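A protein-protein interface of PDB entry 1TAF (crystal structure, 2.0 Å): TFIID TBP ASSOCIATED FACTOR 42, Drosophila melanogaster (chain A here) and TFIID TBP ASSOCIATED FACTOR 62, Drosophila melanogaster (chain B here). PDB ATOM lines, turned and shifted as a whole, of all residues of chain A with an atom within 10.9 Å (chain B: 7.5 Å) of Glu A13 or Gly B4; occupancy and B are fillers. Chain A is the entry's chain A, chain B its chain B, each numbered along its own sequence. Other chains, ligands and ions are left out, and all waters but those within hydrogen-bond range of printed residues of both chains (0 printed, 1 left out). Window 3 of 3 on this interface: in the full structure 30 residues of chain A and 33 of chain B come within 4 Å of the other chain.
The side-chain carboxylate (OE2) of Glu A13 is in hydrogen-bond range of the side-chain hydroxyl (OG) of Ser B5 (2.5 Å).
O of Ser B5 lies within hydrogen-bond range of NZ of Lys B41 (2.7 Å).
O of Leu A11 sits at hydrogen-bond distance from N of Val A16 (2.8 Å).
O of Tyr B3 lies within hydrogen-bond range of NZ of Lys B41 (3.0 Å).
The backbone carbonyl oxygen (O) of Gln A5 is in hydrogen-bond range of the side-chain hydroxyl (OG) of Ser A9 (3.0 Å).
Of the printed residues of chain B, Val A6 touches Ser B6 (3.5 Å).
Printed residues of chain B within 4 Å of Ser A9: Ser B5.
Glu A13 touches just these residues of chain B: Gly B4 and Ser B5.
Of the printed residues of chain A, Gly B4 touches Glu A13.
Ser B5 touches just these residues of chain A: Ser A9 (3.3 Å), Ile A10 (3.96 Å) and Glu A13 (2.5 Å).
Ser B6 touches just one residue of chain A: Val A6 (3.5 Å).
The nearest residue of chain B that does not touch Glu A13 is Lys B41 (4.2 Å).
The nearest printed residue of chain B that does not touch Ile A10 is Val B44 (4.5 Å).
Among the printed residues, merely in contact across the chains: Val A6 with Ser B6 (3.5 Å), Ser A9 with Ser B5 (3.3 Å), Ile A10 with Ser B5 (3.96 Å), Ile A10 with Lys B41 (3.9 Å), Leu A11 with Val B44 (3.7 Å), Glu A13 with Gly B4 (3.6 Å), Leu A14 with Lys B41 (3.4 Å), Leu A14 with Val B44 (3.99 Å) and Val A16 with Val B44 (3.8 Å).
Hydrophobic or aromatic side chains of chain A that line the printed part of chain B: Val A6, Ile A10, Leu A11, Leu A14 and Val A16.
Of the 8 printed residues of chain B, 5 touch a printed residue of chain A.
Printed residues of chain B that touch a printed residue of chain A: Gly B4, Ser B5, Ser B6, Lys B41 and Val B44.
Among the printed residues, 10 pairs touch across the chains.
Among the printed residues, no Asp or Glu carboxylate lies within 4 Å of a Lys or Arg side-chain nitrogen of the other chain.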
ATOM      1  N   ASP A   3     -20.952 -18.718 -20.948  1.00  0.00           N
ATOM      2  CA  ASP A   3     -19.504 -18.516 -21.045  1.00  0.00           C
ATOM      3  C   ASP A   3     -18.748 -19.839 -21.134  1.00  0.00           C
ATOM      4  O   ASP A   3     -17.708 -19.914 -21.793  1.00  0.00           O
ATOM      5  CB  ASP A   3     -18.976 -17.716 -19.850  1.00  0.00           C
ATOM      6  CG  ASP A   3     -19.429 -16.265 -19.859  1.00  0.00           C
ATOM      7  OD1 ASP A   3     -20.103 -15.834 -20.810  1.00  0.00           O
ATOM      8  OD2 ASP A   3     -19.101 -15.538 -18.904  1.00  0.00           O
ATOM      9  N   ALA A   4     -19.261 -20.869 -20.457  1.00  0.00           N
ATOM     10  CA  ALA A   4     -18.635 -22.188 -20.481  1.00  0.00           C
ATOM     11  C   ALA A   4     -18.636 -22.694 -21.913  1.00  0.00           C
ATOM     12  O   ALA A   4     -17.644 -23.257 -22.373  1.00  0.00           O
ATOM     13  CB  ALA A   4     -19.372 -23.155 -19.578  1.00  0.00           C
ATOM     14  N   GLN A   5     -19.742 -22.457 -22.620  1.00  0.00           N
ATOM     15  CA  GLN A   5     -19.888 -22.865 -24.011  1.00  0.00           C
ATOM     16  C   GLN A   5     -18.870 -22.153 -24.898  1.00  0.00           C
ATOM     17  O   GLN A   5     -18.286 -22.760 -25.789  1.00  0.00           O
ATOM     18  CB  GLN A   5     -21.300 -22.569 -24.517  1.00  0.00           C
ATOM     19  CG  GLN A   5     -22.370 -23.502 -23.983  1.00  0.00           C
ATOM     20  CD  GLN A   5     -23.789 -22.964 -24.194  1.00  0.00           C
ATOM     21  OE1 GLN A   5     -24.138 -22.457 -25.276  1.00  0.00           O
ATOM     22  NE2 GLN A   5     -24.612 -23.061 -23.151  1.00  0.00           N
ATOM     23  N   VAL A   6     -18.677 -20.858 -24.669  1.00  0.00           N
ATOM     24  CA  VAL A   6     -17.709 -20.099 -25.450  1.00  0.00           C
ATOM     25  C   VAL A   6     -16.331 -20.712 -25.244  1.00  0.00           C
ATOM     26  O   VAL A   6     -15.574 -20.904 -26.199  1.00  0.00           O
ATOM     27  CB  VAL A   6     -17.642 -18.616 -25.010  1.00  0.00           C
ATOM     28  CG1 VAL A   6     -16.485 -17.909 -25.725  1.00  0.00           C
ATOM     29  CG2 VAL A   6     -18.973 -17.916 -25.302  1.00  0.00           C
ATOM     30  N   ILE A   7     -16.008 -21.020 -23.991  1.00  0.00           N
ATOM     31  CA  ILE A   7     -14.707 -21.597 -23.695  1.00  0.00           C
ATOM     32  C   ILE A   7     -14.541 -22.958 -24.361  1.00  0.00           C
ATOM     33  O   ILE A   7     -13.490 -23.251 -24.917  1.00  0.00           O
ATOM     34  CB  ILE A   7     -14.446 -21.640 -22.184  1.00  0.00           C
ATOM     35  CG1 ILE A   7     -14.233 -20.209 -21.683  1.00  0.00           C
ATOM     36  CG2 ILE A   7     -13.243 -22.527 -21.866  1.00  0.00           C
ATOM     37  CD1 ILE A   7     -14.014 -20.112 -20.230  1.00  0.00           C
ATOM     38  N   MET A   8     -15.607 -23.750 -24.382  1.00  0.00           N
ATOM     39  CA  MET A   8     -15.537 -25.055 -25.014  1.00  0.00           C
ATOM     40  C   MET A   8     -15.332 -24.897 -26.523  1.00  0.00           C
ATOM     41  O   MET A   8     -14.571 -25.653 -27.136  1.00  0.00           O
ATOM     42  CB  MET A   8     -16.786 -25.872 -24.691  1.00  0.00           C
ATOM     43  CG  MET A   8     -16.862 -26.283 -23.230  1.00  0.00           C
ATOM     44  SD  MET A   8     -18.278 -27.347 -22.874  1.00  0.00           S
ATOM     45  CE  MET A   8     -19.465 -26.189 -22.429  1.00  0.00           C
ATOM     46  N   SER A   9     -15.943 -23.861 -27.098  1.00  0.00           N
ATOM     47  CA  SER A   9     -15.814 -23.588 -28.527  1.00  0.00           C
ATOM     48  C   SER A   9     -14.410 -23.122 -28.854  1.00  0.00           C
ATOM     49  O   SER A   9     -13.882 -23.459 -29.912  1.00  0.00           O
ATOM     50  CB  SER A   9     -16.812 -22.523 -28.966  1.00  0.00           C
ATOM     51  OG  SER A   9     -18.141 -22.979 -28.785  1.00  0.00           O
ATOM     52  N   ILE A  10     -13.812 -22.328 -27.963  1.00  0.00           N
ATOM     53  CA  ILE A  10     -12.438 -21.843 -28.176  1.00  0.00           C
ATOM     54  C   ILE A  10     -11.474 -23.038 -28.164  1.00  0.00           C
ATOM     55  O   ILE A  10     -10.579 -23.134 -29.007  1.00  0.00           O
ATOM     56  CB  ILE A  10     -11.997 -20.784 -27.105  1.00  0.00           C
ATOM     57  CG1 ILE A  10     -12.765 -19.462 -27.305  1.00  0.00           C
ATOM     58  CG2 ILE A  10     -10.494 -20.530 -27.198  1.00  0.00           C
ATOM     59  CD1 ILE A  10     -12.384 -18.334 -26.319  1.00  0.00           C
ATOM     60  N   LEU A  11     -11.678 -23.952 -27.215  1.00  0.00           N
ATOM     61  CA  LEU A  11     -10.849 -25.142 -27.110  1.00  0.00           C
ATOM     62  C   LEU A  11     -10.898 -25.955 -28.404  1.00  0.00           C
ATOM     63  O   LEU A  11      -9.867 -26.376 -28.925  1.00  0.00           O
ATOM     64  CB  LEU A  11     -11.294 -25.994 -25.911  1.00  0.00           C
ATOM     65  CG  LEU A  11     -10.872 -25.451 -24.540  1.00  0.00           C
ATOM     66  CD1 LEU A  11     -11.682 -26.096 -23.443  1.00  0.00           C
ATOM     67  CD2 LEU A  11      -9.377 -25.693 -24.304  1.00  0.00           C
ATOM     68  N   LYS A  12     -12.098 -26.132 -28.945  1.00  0.00           N
ATOM     69  CA  LYS A  12     -12.279 -26.879 -30.187  1.00  0.00           C
ATOM     70  C   LYS A  12     -11.681 -26.127 -31.389  1.00  0.00           C
ATOM     71  O   LYS A  12     -10.997 -26.716 -32.224  1.00  0.00           O
ATOM     72  CB  LYS A  12     -13.769 -27.155 -30.411  1.00  0.00           C
ATOM     73  CG  LYS A  12     -14.063 -28.092 -31.566  1.00  0.00           C
ATOM     74  CD  LYS A  12     -15.533 -28.444 -31.617  1.00  0.00           C
ATOM     75  CE  LYS A  12     -15.784 -29.552 -32.638  1.00  0.00           C
ATOM     76  NZ  LYS A  12     -17.194 -30.062 -32.591  1.00  0.00           N
ATOM     77  N   GLU A  13     -11.924 -24.823 -31.461  1.00  0.00           N
ATOM     78  CA  GLU A  13     -11.404 -24.004 -32.553  1.00  0.00           C
ATOM     79  C   GLU A  13      -9.884 -24.000 -32.587  1.00  0.00           C
ATOM     80  O   GLU A  13      -9.287 -23.877 -33.657  1.00  0.00           O
ATOM     81  CB  GLU A  13     -11.905 -22.573 -32.428  1.00  0.00           C
ATOM     82  CG  GLU A  13     -13.357 -22.416 -32.801  1.00  0.00           C
ATOM     83  CD  GLU A  13     -13.996 -21.203 -32.168  1.00  0.00           C
ATOM     84  OE1 GLU A  13     -13.286 -20.403 -31.514  1.00  0.00           O
ATOM     85  OE2 GLU A  13     -15.221 -21.059 -32.309  1.00  0.00           O
ATOM     86  N   LEU A  14      -9.256 -24.110 -31.418  1.00  0.00           N
ATOM     87  CA  LEU A  14      -7.800 -24.121 -31.362  1.00  0.00           C
ATOM     88  C   LEU A  14      -7.249 -25.543 -31.404  1.00  0.00           C
ATOM     89  O   LEU A  14      -6.098 -25.802 -31.057  1.00  0.00           O
ATOM     90  CB  LEU A  14      -7.298 -23.347 -30.147  1.00  0.00           C
ATOM     91  CG  LEU A  14      -7.755 -21.883 -30.105  1.00  0.00           C
ATOM     92  CD1 LEU A  14      -6.996 -21.142 -29.020  1.00  0.00           C
ATOM     93  CD2 LEU A  14      -7.512 -21.226 -31.434  1.00  0.00           C
ATOM     94  N   ASN A  15      -8.098 -26.452 -31.867  1.00  0.00           N
ATOM     95  CA  ASN A  15      -7.767 -27.855 -32.030  1.00  0.00           C
ATOM     96  C   ASN A  15      -7.407 -28.651 -30.796  1.00  0.00           C
ATOM     97  O   ASN A  15      -6.566 -29.558 -30.845  1.00  0.00           O
ATOM     98  CB  ASN A  15      -6.733 -28.036 -33.142  1.00  0.00           C
ATOM     99  CG  ASN A  15      -7.355 -27.916 -34.516  1.00  0.00           C
ATOM    100  OD1 ASN A  15      -8.328 -28.610 -34.822  1.00  0.00           O
ATOM    101  ND2 ASN A  15      -6.829 -27.007 -35.339  1.00  0.00           N
ATOM    102  N   VAL A  16      -8.020 -28.282 -29.677  1.00  0.00           N
ATOM    103  CA  VAL A  16      -7.818 -29.019 -28.444  1.00  0.00           C
ATOM    104  C   VAL A  16      -9.068 -29.900 -28.366  1.00  0.00           C
ATOM    105  O   VAL A  16     -10.106 -29.496 -27.849  1.00  0.00           O
ATOM    106  CB  VAL A  16      -7.706 -28.106 -27.216  1.00  0.00           C
ATOM    107  CG1 VAL A  16      -7.439 -28.957 -25.977  1.00  0.00           C
ATOM    108  CG2 VAL A  16      -6.582 -27.089 -27.419  1.00  0.00           C
ATOM    109  N   GLN A  17      -8.954 -31.080 -28.967  1.00  0.00           N
ATOM    110  CA  GLN A  17     -10.032 -32.060 -29.048  1.00  0.00           C
ATOM    111  C   GLN A  17     -10.390 -32.763 -27.741  1.00  0.00           C
ATOM    112  O   GLN A  17     -11.534 -33.170 -27.540  1.00  0.00           O
ATOM    113  CB  GLN A  17      -9.685 -33.075 -30.130  1.00  0.00           C
ATOM    114  CG  GLN A  17      -9.409 -32.407 -31.472  1.00  0.00           C
ATOM    115  CD  GLN A  17      -8.855 -33.364 -32.494  1.00  0.00           C
ATOM    116  OE1 GLN A  17      -9.516 -34.333 -32.878  1.00  0.00           O
ATOM    117  NE2 GLN A  17      -7.628 -33.103 -32.945  1.00  0.00           N
ATOM    118  N   GLU A  18      -9.416 -32.904 -26.852  1.00  0.00           N
ATOM    119  CA  GLU A  18      -9.664 -33.536 -25.565  1.00  0.00           C
ATOM    120  C   GLU A  18      -8.997 -32.731 -24.466  1.00  0.00           C
ATOM    121  O   GLU A  18      -7.872 -32.263 -24.624  1.00  0.00           O
ATOM    122  CB  GLU A  18      -9.104 -34.951 -25.550  1.00  0.00           C
ATOM    123  CG  GLU A  18      -9.735 -35.900 -26.545  1.00  0.00           C
ATOM    124  CD  GLU A  18      -9.126 -37.285 -26.446  1.00  0.00           C
ATOM    125  OE1 GLU A  18      -7.916 -37.423 -26.726  1.00  0.00           O
ATOM    126  OE2 GLU A  18      -9.842 -38.224 -26.057  1.00  0.00           O
ATOM    127  N   TYR A  19      -9.694 -32.586 -23.347  1.00  0.00           N
ATOM    128  CA  TYR A  19      -9.178 -31.844 -22.205  1.00  0.00           C
ATOM    129  C   TYR A  19      -9.879 -32.284 -20.926  1.00  0.00           C
ATOM    130  O   TYR A  19     -10.993 -32.817 -20.971  1.00  0.00           O
ATOM    131  CB  TYR A  19      -9.385 -30.337 -22.422  1.00  0.00           C
ATOM    132  CG  TYR A  19     -10.786 -29.951 -22.854  1.00  0.00           C
ATOM    133  CD1 TYR A  19     -11.793 -29.731 -21.916  1.00  0.00           C
ATOM    134  CD2 TYR A  19     -11.099 -29.812 -24.200  1.00  0.00           C
ATOM    135  CE1 TYR A  19     -13.077 -29.379 -22.305  1.00  0.00           C
ATOM    136  CE2 TYR A  19     -12.384 -29.464 -24.605  1.00  0.00           C
ATOM    137  CZ  TYR A  19     -13.365 -29.246 -23.653  1.00  0.00           C
ATOM    138  OH  TYR A  19     -14.635 -28.878 -24.050  1.00  0.00           O
ATOM    139  N   LEU B   2     -11.877 -10.171 -34.273  1.00  0.00           N
ATOM    140  CA  LEU B   2     -11.558 -11.538 -33.869  1.00  0.00           C
ATOM    141  C   LEU B   2     -12.287 -12.614 -34.660  1.00  0.00           C
ATOM    142  O   LEU B   2     -13.463 -12.469 -34.984  1.00  0.00           O
ATOM    143  CB  LEU B   2     -11.858 -11.735 -32.377  1.00  0.00           C
ATOM    144  CG  LEU B   2     -10.734 -11.565 -31.353  1.00  0.00           C
ATOM    145  CD1 LEU B   2     -11.291 -11.765 -29.955  1.00  0.00           C
ATOM    146  CD2 LEU B   2      -9.632 -12.575 -31.617  1.00  0.00           C
ATOM    147  N   TYR B   3     -11.560 -13.663 -35.022  1.00  0.00           N
ATOM    148  CA  TYR B   3     -12.155 -14.791 -35.714  1.00  0.00           C
ATOM    149  C   TYR B   3     -12.382 -15.815 -34.607  1.00  0.00           C
ATOM    150  O   TYR B   3     -11.739 -15.757 -33.551  1.00  0.00           O
ATOM    151  CB  TYR B   3     -11.219 -15.365 -36.773  1.00  0.00           C
ATOM    152  CG  TYR B   3     -10.906 -14.434 -37.933  1.00  0.00           C
ATOM    153  CD1 TYR B   3     -11.891 -13.619 -38.504  1.00  0.00           C
ATOM    154  CD2 TYR B   3      -9.622 -14.392 -38.478  1.00  0.00           C
ATOM    155  CE1 TYR B   3     -11.595 -12.784 -39.596  1.00  0.00           C
ATOM    156  CE2 TYR B   3      -9.315 -13.574 -39.560  1.00  0.00           C
ATOM    157  CZ  TYR B   3     -10.298 -12.774 -40.119  1.00  0.00           C
ATOM    158  OH  TYR B   3      -9.972 -11.991 -41.214  1.00  0.00           O
ATOM    159  N   GLY B   4     -13.321 -16.724 -34.828  1.00  0.00           N
ATOM    160  CA  GLY B   4     -13.611 -17.726 -33.827  1.00  0.00           C
ATOM    161  C   GLY B   4     -14.546 -17.181 -32.775  1.00  0.00           C
ATOM    162  O   GLY B   4     -15.137 -16.122 -32.953  1.00  0.00           O
ATOM    163  N   SER B   5     -14.665 -17.899 -31.667  1.00  0.00           N
ATOM    164  CA  SER B   5     -15.545 -17.502 -30.586  1.00  0.00           C
ATOM    165  C   SER B   5     -14.965 -16.467 -29.622  1.00  0.00           C
ATOM    166  O   SER B   5     -13.753 -16.305 -29.488  1.00  0.00           O
ATOM    167  CB  SER B   5     -15.983 -18.734 -29.812  1.00  0.00           C
ATOM    168  OG  SER B   5     -16.555 -19.681 -30.694  1.00  0.00           O
ATOM    169  N   SER B   6     -15.856 -15.778 -28.928  1.00  0.00           N
ATOM    170  CA  SER B   6     -15.440 -14.785 -27.966  1.00  0.00           C
ATOM    171  C   SER B   6     -16.498 -14.604 -26.895  1.00  0.00           C
ATOM    172  O   SER B   6     -17.673 -14.879 -27.110  1.00  0.00           O
ATOM    173  CB  SER B   6     -15.153 -13.457 -28.669  1.00  0.00           C
ATOM    174  OG  SER B   6     -16.304 -12.967 -29.311  1.00  0.00           O
ATOM    175  N   LYS B  41      -7.521 -17.302 -25.794  1.00  0.00           N
ATOM    176  CA  LYS B  41      -6.957 -18.026 -26.931  1.00  0.00           C
ATOM    177  C   LYS B  41      -5.448 -18.201 -26.742  1.00  0.00           C
ATOM    178  O   LYS B  41      -4.918 -19.272 -27.021  1.00  0.00           O
ATOM    179  CB  LYS B  41      -7.294 -17.307 -28.238  1.00  0.00           C
ATOM    180  CG  LYS B  41      -8.809 -17.297 -28.573  1.00  0.00           C
ATOM    181  CD  LYS B  41      -9.112 -16.225 -29.619  1.00  0.00           C
ATOM    182  CE  LYS B  41     -10.607 -15.896 -29.753  1.00  0.00           C
ATOM    183  NZ  LYS B  41     -11.365 -16.698 -30.761  1.00  0.00           N
ATOM    184  N   VAL B  44      -4.885 -20.904 -23.923  1.00  0.00           N
ATOM    185  CA  VAL B  44      -5.180 -22.229 -24.455  1.00  0.00           C
ATOM    186  C   VAL B  44      -4.093 -22.674 -25.444  1.00  0.00           C
ATOM    187  O   VAL B  44      -3.638 -23.819 -25.412  1.00  0.00           O
ATOM    188  CB  VAL B  44      -6.566 -22.253 -25.139  1.00  0.00           C
ATOM    189  CG1 VAL B  44      -6.787 -23.574 -25.863  1.00  0.00           C
ATOM    190  CG2 VAL B  44      -7.666 -22.039 -24.095  1.00  0.00           C
ATOM    191  N   GLN B  45      -3.680 -21.761 -26.315  1.00  0.00           N
ATOM    192  CA  GLN B  45      -2.638 -22.058 -27.295  1.00  0.00           C
ATOM    193  C   GLN B  45      -1.323 -22.465 -26.614  1.00  0.00           C
ATOM    194  O   GLN B  45      -0.749 -23.491 -26.946  1.00  0.00           O
ATOM    195  CB  GLN B  45      -2.418 -20.843 -28.198  1.00  0.00           C
ATOM    196  CG  GLN B  45      -1.394 -21.049 -29.318  1.00  0.00           C
ATOM    197  CD  GLN B  45      -1.800 -22.141 -30.291  1.00  0.00           C
ATOM    198  OE1 GLN B  45      -2.881 -22.104 -30.895  1.00  0.00           O
ATOM    199  NE2 GLN B  45      -0.931 -23.128 -30.442  1.00  0.00           N
